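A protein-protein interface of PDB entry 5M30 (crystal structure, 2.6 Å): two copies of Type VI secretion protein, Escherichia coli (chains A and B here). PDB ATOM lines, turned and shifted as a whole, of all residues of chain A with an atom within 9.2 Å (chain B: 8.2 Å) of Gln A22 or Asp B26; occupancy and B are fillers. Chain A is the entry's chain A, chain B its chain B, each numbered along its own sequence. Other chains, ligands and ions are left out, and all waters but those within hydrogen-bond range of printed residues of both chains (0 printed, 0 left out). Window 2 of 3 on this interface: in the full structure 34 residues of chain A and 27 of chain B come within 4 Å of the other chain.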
ATOM      1  N   PHE A  19      19.863  -8.060  36.828  1.00  0.00           N
ATOM      2  CA  PHE A  19      18.457  -8.095  37.211  1.00  0.00           C
ATOM      3  C   PHE A  19      17.556  -8.104  35.945  1.00  0.00           C
ATOM      4  O   PHE A  19      17.308  -9.176  35.378  1.00  0.00           O
ATOM      5  CB  PHE A  19      18.151  -6.922  38.172  1.00  0.00           C
ATOM      6  CG  PHE A  19      16.865  -7.045  38.951  1.00  0.00           C
ATOM      7  N   GLN A  20      17.109  -6.913  35.489  1.00  0.00           N
ATOM      8  CA  GLN A  20      16.272  -6.722  34.296  1.00  0.00           C
ATOM      9  C   GLN A  20      17.131  -6.713  33.023  1.00  0.00           C
ATOM     10  O   GLN A  20      16.621  -7.004  31.936  1.00  0.00           O
ATOM     11  CB  GLN A  20      15.490  -5.402  34.403  1.00  0.00           C
ATOM     12  N   GLN A  21      18.438  -6.369  33.172  1.00  0.00           N
ATOM     13  CA  GLN A  21      19.434  -6.281  32.099  1.00  0.00           C
ATOM     14  C   GLN A  21      19.713  -7.630  31.434  1.00  0.00           C
ATOM     15  O   GLN A  21      19.879  -7.672  30.213  1.00  0.00           O
ATOM     16  CB  GLN A  21      20.735  -5.647  32.617  1.00  0.00           C
ATOM     17  N   GLN A  22      19.765  -8.727  32.233  1.00  0.00           N
ATOM     18  CA  GLN A  22      20.006 -10.095  31.745  1.00  0.00           C
ATOM     19  C   GLN A  22      18.814 -10.596  30.929  1.00  0.00           C
ATOM     20  O   GLN A  22      19.031 -11.154  29.856  1.00  0.00           O
ATOM     21  CB  GLN A  22      20.339 -11.072  32.895  1.00  0.00           C
ATOM     22  CG  GLN A  22      21.227 -12.266  32.467  1.00  0.00           C
ATOM     23  CD  GLN A  22      20.568 -13.641  32.407  1.00  0.00           C
ATOM     24  OE1 GLN A  22      21.241 -14.680  32.501  1.00  0.00           O
ATOM     25  NE2 GLN A  22      19.255 -13.698  32.203  1.00  0.00           N
ATOM     26  N   ALA A  23      17.567 -10.360  31.422  1.00  0.00           N
ATOM     27  CA  ALA A  23      16.302 -10.715  30.764  1.00  0.00           C
ATOM     28  C   ALA A  23      16.219 -10.042  29.384  1.00  0.00           C
ATOM     29  O   ALA A  23      15.804 -10.679  28.415  1.00  0.00           O
ATOM     30  CB  ALA A  23      15.126 -10.293  31.633  1.00  0.00           C
ATOM     31  N   ALA A  24      16.664  -8.768  29.296  1.00  0.00           N
ATOM     32  CA  ALA A  24      16.742  -8.012  28.049  1.00  0.00           C
ATOM     33  C   ALA A  24      17.857  -8.629  27.191  1.00  0.00           C
ATOM     34  O   ALA A  24      18.928  -8.957  27.723  1.00  0.00           O
ATOM     35  CB  ALA A  24      17.060  -6.549  28.345  1.00  0.00           C
ATOM     36  N   TRP A  25      17.576  -8.854  25.883  1.00  0.00           N
ATOM     37  CA  TRP A  25      18.496  -9.413  24.871  1.00  0.00           C
ATOM     38  C   TRP A  25      18.803 -10.937  25.130  1.00  0.00           C
ATOM     39  O   TRP A  25      19.266 -11.615  24.206  1.00  0.00           O
ATOM     40  CB  TRP A  25      19.761  -8.510  24.673  1.00  0.00           C
ATOM     41  CG  TRP A  25      21.071  -9.177  24.336  1.00  0.00           C
ATOM     42  CD1 TRP A  25      21.941  -9.744  25.219  1.00  0.00           C
ATOM     43  CD2 TRP A  25      21.711  -9.236  23.048  1.00  0.00           C
ATOM     44  NE1 TRP A  25      23.044 -10.226  24.554  1.00  0.00           N
ATOM     45  CE2 TRP A  25      22.931  -9.926  23.221  1.00  0.00           C
ATOM     46  CE3 TRP A  25      21.350  -8.820  21.756  1.00  0.00           C
ATOM     47  CZ2 TRP A  25      23.799 -10.198  22.156  1.00  0.00           C
ATOM     48  CZ3 TRP A  25      22.211  -9.092  20.702  1.00  0.00           C
ATOM     49  CH2 TRP A  25      23.417  -9.776  20.906  1.00  0.00           C
ATOM     50  N   ASP A  26      18.442 -11.486  26.323  1.00  0.00           N
ATOM     51  CA  ASP A  26      18.518 -12.930  26.617  1.00  0.00           C
ATOM     52  C   ASP A  26      17.357 -13.547  25.814  1.00  0.00           C
ATOM     53  O   ASP A  26      17.495 -14.605  25.201  1.00  0.00           O
ATOM     54  CB  ASP A  26      18.271 -13.192  28.113  1.00  0.00           C
ATOM     55  CG  ASP A  26      19.002 -14.381  28.712  1.00  0.00           C
ATOM     56  OD1 ASP A  26      20.255 -14.412  28.637  1.00  0.00           O
ATOM     57  OD2 ASP A  26      18.331 -15.233  29.343  1.00  0.00           O
ATOM     58  N   VAL A  27      16.216 -12.824  25.813  1.00  0.00           N
ATOM     59  CA  VAL A  27      14.982 -13.089  25.080  1.00  0.00           C
ATOM     60  C   VAL A  27      15.296 -12.997  23.570  1.00  0.00           C
ATOM     61  O   VAL A  27      14.800 -13.827  22.806  1.00  0.00           O
ATOM     62  CB  VAL A  27      13.869 -12.122  25.575  1.00  0.00           C
ATOM     63  CG1 VAL A  27      12.875 -11.745  24.489  1.00  0.00           C
ATOM     64  CG2 VAL A  27      13.148 -12.701  26.789  1.00  0.00           C
ATOM     65  N   HIS A  28      16.179 -12.055  23.171  1.00  0.00           N
ATOM     66  CA  HIS A  28      16.624 -11.899  21.784  1.00  0.00           C
ATOM     67  C   HIS A  28      17.452 -13.097  21.306  1.00  0.00           C
ATOM     68  O   HIS A  28      17.359 -13.476  20.142  1.00  0.00           O
ATOM     69  CB  HIS A  28      17.412 -10.604  21.577  1.00  0.00           C
ATOM     70  CG  HIS A  28      17.866 -10.400  20.159  1.00  0.00           C
ATOM     71  ND1 HIS A  28      16.982 -10.012  19.169  1.00  0.00           N
ATOM     72  CD2 HIS A  28      19.095 -10.546  19.607  1.00  0.00           C
ATOM     73  CE1 HIS A  28      17.686  -9.943  18.049  1.00  0.00           C
ATOM     74  NE2 HIS A  28      18.964 -10.245  18.261  1.00  0.00           N
ATOM     75  N   LEU A  29      18.257 -13.674  22.192  1.00  0.00           N
ATOM     76  CA  LEU A  29      19.072 -14.846  21.904  1.00  0.00           C
ATOM     77  C   LEU A  29      18.163 -16.058  21.644  1.00  0.00           C
ATOM     78  O   LEU A  29      18.358 -16.763  20.646  1.00  0.00           O
ATOM     79  CB  LEU A  29      20.009 -15.129  23.089  1.00  0.00           C
ATOM     80  CG  LEU A  29      21.501 -14.854  22.893  1.00  0.00           C
ATOM     81  CD1 LEU A  29      21.793 -13.366  22.720  1.00  0.00           C
ATOM     82  CD2 LEU A  29      22.309 -15.427  24.049  1.00  0.00           C
ATOM     83  N   ALA A  30      17.149 -16.295  22.517  1.00  0.00           N
ATOM     84  CA  ALA A  30      16.218 -17.422  22.336  1.00  0.00           C
ATOM     85  C   ALA A  30      15.372 -17.230  21.071  1.00  0.00           C
ATOM     86  O   ALA A  30      15.173 -18.201  20.331  1.00  0.00           O
ATOM     87  CB  ALA A  30      15.332 -17.586  23.558  1.00  0.00           C
ATOM     88  N   ARG A  67       3.358 -15.859  23.865  1.00  0.00           N
ATOM     89  CA  ARG A  67       4.683 -15.390  23.481  1.00  0.00           C
ATOM     90  C   ARG A  67       4.521 -14.223  22.512  1.00  0.00           C
ATOM     91  O   ARG A  67       3.832 -14.352  21.503  1.00  0.00           O
ATOM     92  CB  ARG A  67       5.497 -16.529  22.873  1.00  0.00           C
ATOM     93  CG  ARG A  67       6.924 -16.155  22.550  1.00  0.00           C
ATOM     94  CD  ARG A  67       7.635 -17.349  22.009  1.00  0.00           C
ATOM     95  NE  ARG A  67       8.128 -18.185  23.095  1.00  0.00           N
ATOM     96  CZ  ARG A  67       9.399 -18.252  23.451  1.00  0.00           C
ATOM     97  NH1 ARG A  67      10.319 -17.549  22.792  1.00  0.00           N
ATOM     98  NH2 ARG A  67       9.771 -19.036  24.452  1.00  0.00           N
ATOM     99  N   LEU A 106       9.799  -2.746  25.398  1.00  0.00           N
ATOM    100  CA  LEU A 106      10.995  -2.570  26.192  1.00  0.00           C
ATOM    101  C   LEU A 106      11.750  -1.375  25.619  1.00  0.00           C
ATOM    102  O   LEU A 106      11.944  -1.298  24.405  1.00  0.00           O
ATOM    103  CB  LEU A 106      11.844  -3.827  26.142  1.00  0.00           C
ATOM    104  CG  LEU A 106      12.808  -3.930  27.306  1.00  0.00           C
ATOM    105  CD1 LEU A 106      12.291  -4.906  28.348  1.00  0.00           C
ATOM    106  CD2 LEU A 106      14.214  -4.269  26.819  1.00  0.00           C
ATOM    107  N   TRP A 125       7.636  -3.203  33.383  1.00  0.00           N
ATOM    108  CA  TRP A 125       7.577  -3.766  34.732  1.00  0.00           C
ATOM    109  C   TRP A 125       7.059  -2.872  35.821  1.00  0.00           C
ATOM    110  O   TRP A 125       7.179  -1.660  35.745  1.00  0.00           O
ATOM    111  CB  TRP A 125       8.973  -4.247  35.161  1.00  0.00           C
ATOM    112  CG  TRP A 125       9.494  -5.410  34.377  1.00  0.00           C
ATOM    113  CD1 TRP A 125       9.018  -6.691  34.394  1.00  0.00           C
ATOM    114  CD2 TRP A 125      10.637  -5.415  33.514  1.00  0.00           C
ATOM    115  NE1 TRP A 125       9.786  -7.489  33.581  1.00  0.00           N
ATOM    116  CE2 TRP A 125      10.780  -6.731  33.016  1.00  0.00           C
ATOM    117  CE3 TRP A 125      11.562  -4.434  33.110  1.00  0.00           C
ATOM    118  CZ2 TRP A 125      11.808  -7.091  32.134  1.00  0.00           C
ATOM    119  CZ3 TRP A 125      12.585  -4.796  32.243  1.00  0.00           C
ATOM    120  CH2 TRP A 125      12.698  -6.108  31.765  1.00  0.00           C
ATOM    121  N   LEU A 146      10.418  -7.912  40.065  1.00  0.00           N
ATOM    122  CA  LEU A 146       9.755  -7.379  38.868  1.00  0.00           C
ATOM    123  C   LEU A 146       8.533  -8.199  38.456  1.00  0.00           C
ATOM    124  O   LEU A 146       8.579  -9.434  38.423  1.00  0.00           O
ATOM    125  CB  LEU A 146      10.733  -7.368  37.673  1.00  0.00           C
ATOM    126  CG  LEU A 146      12.051  -6.618  37.802  1.00  0.00           C
ATOM    127  CD1 LEU A 146      13.004  -7.047  36.701  1.00  0.00           C
ATOM    128  CD2 LEU A 146      11.835  -5.108  37.781  1.00  0.00           C
ATOM    129  N   GLN B  20      20.672 -20.086  41.457  1.00  0.00           N
ATOM    130  CA  GLN B  20      19.947 -21.249  40.957  1.00  0.00           C
ATOM    131  C   GLN B  20      18.637 -20.818  40.263  1.00  0.00           C
ATOM    132  O   GLN B  20      18.121 -21.553  39.424  1.00  0.00           O
ATOM    133  CB  GLN B  20      19.633 -22.184  42.134  1.00  0.00           C
ATOM    134  N   GLN B  21      18.093 -19.638  40.633  1.00  0.00           N
ATOM    135  CA  GLN B  21      16.849 -19.075  40.104  1.00  0.00           C
ATOM    136  C   GLN B  21      16.933 -18.752  38.610  1.00  0.00           C
ATOM    137  O   GLN B  21      15.971 -19.005  37.872  1.00  0.00           O
ATOM    138  CB  GLN B  21      16.433 -17.837  40.916  1.00  0.00           C
ATOM    139  N   GLN B  22      18.093 -18.216  38.166  1.00  0.00           N
ATOM    140  CA  GLN B  22      18.334 -17.841  36.771  1.00  0.00           C
ATOM    141  C   GLN B  22      18.470 -19.073  35.889  1.00  0.00           C
ATOM    142  O   GLN B  22      17.862 -19.111  34.813  1.00  0.00           O
ATOM    143  CB  GLN B  22      19.560 -16.910  36.635  1.00  0.00           C
ATOM    144  N   ALA B  23      19.250 -20.079  36.346  1.00  0.00           N
ATOM    145  CA  ALA B  23      19.468 -21.343  35.633  1.00  0.00           C
ATOM    146  C   ALA B  23      18.143 -22.015  35.240  1.00  0.00           C
ATOM    147  O   ALA B  23      17.964 -22.306  34.060  1.00  0.00           O
ATOM    148  CB  ALA B  23      20.330 -22.295  36.459  1.00  0.00           C
ATOM    149  N   ALA B  24      17.192 -22.166  36.199  1.00  0.00           N
ATOM    150  CA  ALA B  24      15.873 -22.779  35.993  1.00  0.00           C
ATOM    151  C   ALA B  24      15.046 -22.175  34.846  1.00  0.00           C
ATOM    152  O   ALA B  24      14.484 -22.912  34.031  1.00  0.00           O
ATOM    153  CB  ALA B  24      15.070 -22.736  37.283  1.00  0.00           C
ATOM    154  N   TRP B  25      14.949 -20.848  34.804  1.00  0.00           N
ATOM    155  CA  TRP B  25      14.143 -20.149  33.823  1.00  0.00           C
ATOM    156  C   TRP B  25      14.725 -20.198  32.440  1.00  0.00           C
ATOM    157  O   TRP B  25      13.971 -20.257  31.458  1.00  0.00           O
ATOM    158  CB  TRP B  25      13.882 -18.704  34.259  1.00  0.00           C
ATOM    159  CG  TRP B  25      12.757 -18.046  33.512  1.00  0.00           C
ATOM    160  CD1 TRP B  25      12.851 -16.980  32.665  1.00  0.00           C
ATOM    161  CD2 TRP B  25      11.363 -18.425  33.531  1.00  0.00           C
ATOM    162  NE1 TRP B  25      11.606 -16.661  32.161  1.00  0.00           N
ATOM    163  CE2 TRP B  25      10.676 -17.540  32.667  1.00  0.00           C
ATOM    164  CE3 TRP B  25      10.626 -19.429  34.202  1.00  0.00           C
ATOM    165  CZ2 TRP B  25       9.287 -17.632  32.443  1.00  0.00           C
ATOM    166  CZ3 TRP B  25       9.254 -19.513  33.987  1.00  0.00           C
ATOM    167  CH2 TRP B  25       8.599 -18.624  33.119  1.00  0.00           C
ATOM    168  N   ASP B  26      16.064 -20.182  32.354  1.00  0.00           N
ATOM    169  CA  ASP B  26      16.755 -20.204  31.070  1.00  0.00           C
ATOM    170  C   ASP B  26      16.714 -21.624  30.439  1.00  0.00           C
ATOM    171  O   ASP B  26      16.700 -21.737  29.210  1.00  0.00           O
ATOM    172  CB  ASP B  26      18.167 -19.593  31.179  1.00  0.00           C
ATOM    173  CG  ASP B  26      18.275 -18.177  31.788  1.00  0.00           C
ATOM    174  OD1 ASP B  26      17.228 -17.623  32.240  1.00  0.00           O
ATOM    175  OD2 ASP B  26      19.408 -17.629  31.827  1.00  0.00           O
ATOM    176  N   VAL B  27      16.596 -22.690  31.279  1.00  0.00           N
ATOM    177  CA  VAL B  27      16.357 -24.073  30.854  1.00  0.00           C
ATOM    178  C   VAL B  27      14.912 -24.125  30.270  1.00  0.00           C
ATOM    179  O   VAL B  27      14.701 -24.712  29.202  1.00  0.00           O
ATOM    180  CB  VAL B  27      16.587 -25.072  32.023  1.00  0.00           C
ATOM    181  CG1 VAL B  27      15.793 -26.356  31.854  1.00  0.00           C
ATOM    182  CG2 VAL B  27      18.067 -25.381  32.201  1.00  0.00           C
ATOM    183  N   HIS B  28      13.952 -23.445  30.938  1.00  0.00           N
ATOM    184  CA  HIS B  28      12.554 -23.342  30.507  1.00  0.00           C
ATOM    185  C   HIS B  28      12.424 -22.567  29.206  1.00  0.00           C
ATOM    186  O   HIS B  28      11.577 -22.907  28.380  1.00  0.00           O
ATOM    187  CB  HIS B  28      11.688 -22.701  31.598  1.00  0.00           C
ATOM    188  CG  HIS B  28      10.246 -22.559  31.210  1.00  0.00           C
ATOM    189  ND1 HIS B  28       9.405 -23.665  31.137  1.00  0.00           N
ATOM    190  CD2 HIS B  28       9.551 -21.453  30.839  1.00  0.00           C
ATOM    191  CE1 HIS B  28       8.225 -23.192  30.756  1.00  0.00           C
ATOM    192  NE2 HIS B  28       8.264 -21.868  30.559  1.00  0.00           N
ATOM    193  N   LEU B  29      13.238 -21.515  29.034  1.00  0.00           N
ATOM    194  CA  LEU B  29      13.250 -20.692  27.832  1.00  0.00           C
ATOM    195  C   LEU B  29      13.714 -21.524  26.644  1.00  0.00           C
ATOM    196  O   LEU B  29      13.063 -21.524  25.606  1.00  0.00           O
ATOM    197  CB  LEU B  29      14.177 -19.485  28.053  1.00  0.00           C
ATOM    198  CG  LEU B  29      13.536 -18.082  28.114  1.00  0.00           C
ATOM    199  CD1 LEU B  29      12.624 -17.933  29.310  1.00  0.00           C
ATOM    200  CD2 LEU B  29      14.617 -17.003  28.181  1.00  0.00           C
ATOM    201  N   ALA B  30      14.809 -22.263  26.805  1.00  0.00           N
ATOM    202  CA  ALA B  30      15.348 -23.129  25.770  1.00  0.00           C
ATOM    203  C   ALA B  30      14.382 -24.293  25.460  1.00  0.00           C
ATOM    204  O   ALA B  30      14.266 -24.703  24.302  1.00  0.00           O
ATOM    205  CB  ALA B  30      16.684 -23.673  26.233  1.00  0.00           C
ATOM    206  N   ASP B  31      13.733 -24.856  26.497  1.00  0.00           N
ATOM    207  CA  ASP B  31      12.779 -25.939  26.296  1.00  0.00           C
ATOM    208  C   ASP B  31      11.579 -25.459  25.502  1.00  0.00           C
ATOM    209  O   ASP B  31      11.196 -26.115  24.537  1.00  0.00           O
ATOM    210  CB  ASP B  31      12.326 -26.546  27.620  1.00  0.00           C
ATOM    211  CG  ASP B  31      11.529 -27.833  27.452  1.00  0.00           C
ATOM    212  OD1 ASP B  31      12.079 -28.825  26.827  1.00  0.00           O
ATOM    213  OD2 ASP B  31      10.400 -27.898  27.998  1.00  0.00           O
ATOM    214  N   SER B  32      11.015 -24.294  25.891  1.00  0.00           N
ATOM    215  CA  SER B  32       9.875 -23.691  25.230  1.00  0.00           C
ATOM    216  C   SER B  32      10.149 -23.406  23.762  1.00  0.00           C
ATOM    217  O   SER B  32       9.239 -23.533  22.949  1.00  0.00           O
ATOM    218  CB  SER B  32       9.404 -22.451  25.983  1.00  0.00           C
ATOM    219  OG  SER B  32      10.377 -21.426  25.953  1.00  0.00           O
ATOM    220  N   VAL B  33      11.407 -23.088  23.414  1.00  0.00           N
ATOM    221  CA  VAL B  33      11.836 -22.856  22.037  1.00  0.00           C
ATOM    222  C   VAL B  33      11.959 -24.186  21.305  1.00  0.00           C
ATOM    223  O   VAL B  33      11.520 -24.275  20.172  1.00  0.00           O
ATOM    224  CB  VAL B  33      13.123 -21.991  21.943  1.00  0.00           C
ATOM    225  CG1 VAL B  33      13.677 -21.956  20.504  1.00  0.00           C
ATOM    226  CG2 VAL B  33      12.873 -20.572  22.473  1.00  0.00           C
ATOM    227  N   ARG B  67      19.553 -35.274  27.987  1.00  0.00           N
ATOM    228  CA  ARG B  67      18.674 -34.115  28.133  1.00  0.00           C
ATOM    229  C   ARG B  67      17.360 -34.576  28.742  1.00  0.00           C
ATOM    230  O   ARG B  67      16.678 -35.443  28.199  1.00  0.00           O
ATOM    231  CB  ARG B  67      18.452 -33.460  26.774  1.00  0.00           C
ATOM    232  CG  ARG B  67      17.487 -32.314  26.790  1.00  0.00           C
ATOM    233  CD  ARG B  67      17.841 -31.277  25.766  1.00  0.00           C
ATOM    234  NE  ARG B  67      16.700 -30.387  25.661  1.00  0.00           N
ATOM    235  CZ  ARG B  67      16.757 -29.066  25.750  1.00  0.00           C
ATOM    236  NH1 ARG B  67      17.933 -28.451  25.883  1.00  0.00           N
ATOM    237  NH2 ARG B  67      15.641 -28.341  25.662  1.00  0.00           N
ATOM    238  N   ASP B  70      12.430 -31.726  31.097  1.00  0.00           N
ATOM    239  CA  ASP B  70      12.170 -30.362  31.574  1.00  0.00           C
ATOM    240  C   ASP B  70      13.112 -29.371  30.894  1.00  0.00           C
ATOM    241  O   ASP B  70      13.092 -28.183  31.218  1.00  0.00           O
ATOM    242  CB  ASP B  70      12.370 -30.276  33.091  1.00  0.00           C
ATOM    243  CG  ASP B  70      13.834 -30.282  33.519  1.00  0.00           C
ATOM    244  OD1 ASP B  70      14.652 -30.934  32.839  1.00  0.00           O
ATOM    245  OD2 ASP B  70      14.135 -29.728  34.577  1.00  0.00           O
ATOM    246  N   GLY B  71      13.978 -29.864  30.026  1.00  0.00           N
ATOM    247  CA  GLY B  71      14.937 -29.043  29.303  1.00  0.00           C
ATOM    248  C   GLY B  71      16.372 -29.090  29.780  1.00  0.00           C
ATOM    249  O   GLY B  71      17.235 -28.544  29.106  1.00  0.00           O
ATOM    250  N   THR B  72      16.633 -29.688  30.956  1.00  0.00           N
ATOM    251  CA  THR B  72      17.954 -29.792  31.569  1.00  0.00           C
ATOM    252  C   THR B  72      18.879 -30.731  30.858  1.00  0.00           C
ATOM    253  O   THR B  72      18.660 -31.948  30.838  1.00  0.00           O
ATOM    254  CB  THR B  72      17.858 -30.207  33.024  1.00  0.00           C
ATOM    255  OG1 THR B  72      16.867 -29.393  33.652  1.00  0.00           O
ATOM    256  CG2 THR B  72      19.208 -30.130  33.751  1.00  0.00           C
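The guanidinium group (NH2) of Arg A67 lies within hydrogen-bond range of the side-chain hydroxyl (OG) of Ser B32 (2.9 Å).
O of Leu B29 sits at hydrogen-bond distance from OG of Ser B32 (2.7 Å). The side-chain carboxylate (OD2) of Asp A26 sits at hydrogen-bond distance from the side-chain amide nitrogen (NE2) of Gln A22 (3.4 Å). The backbone carbonyl oxygen (O) of His B28 sits at hydrogen-bond distance from the side-chain hydroxyl (OG) of Ser B32 (3.1 Å).
Gln A22 touches Asp B26. OD2 of Asp A26 touches OD2 of Asp B26, 3.6 Å away. Ala A30 touches Val B33 (O to CG2, 3.9 Å). NH1 of Arg A67 touches CG2 of Val B33, 3.97 Å away.
No residue of chain B comes within 4 Å of Gln A21. Of chain B, only Asp B26 (3.5 Å) comes within 4 Å of Gln A22. Trp A25 touches none of the printed residues of chain B. Of the printed residues of chain B, Asp A26 touches Asp B26 (3.6 Å). Printed residues of chain B within 4 Å of Ala A30: Val B33. Of the printed residues of chain B, Arg A67 touches Ser B32 and Val B33. No residue of chain A comes within 4 Å of Val B27. Leu B29 touches none of the printed residues of chain A. Ala B30 touches none of the printed residues of chain A. Of the printed residues of chain A, Ser B32 touches Arg A67. The nearest printed residue of chain A that does not touch Asp B26 is Ala A23 (7.1 Å). The nearest printed residue of chain A that does not touch Ser B32 is Ala A30 (6.7 Å).
Printed residues of chain B that touch a printed residue of chain A: Asp B26, Ser B32 and Val B33. Hydrophobic or aromatic side chains of chain B within 4 Å of the printed part of chain A: Val B33.
Gln A22 touches Asp B26, but with the chains exchanged Asp A26 does not touch Gln B22 (6.7 Å). Asp B26 touches its own counterpart, Asp A26. 12 positions are printed for both chains. Of the 5 pairs that touch across the chains among the printed residues, 1 has its exchanged pair printed and touching as well.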
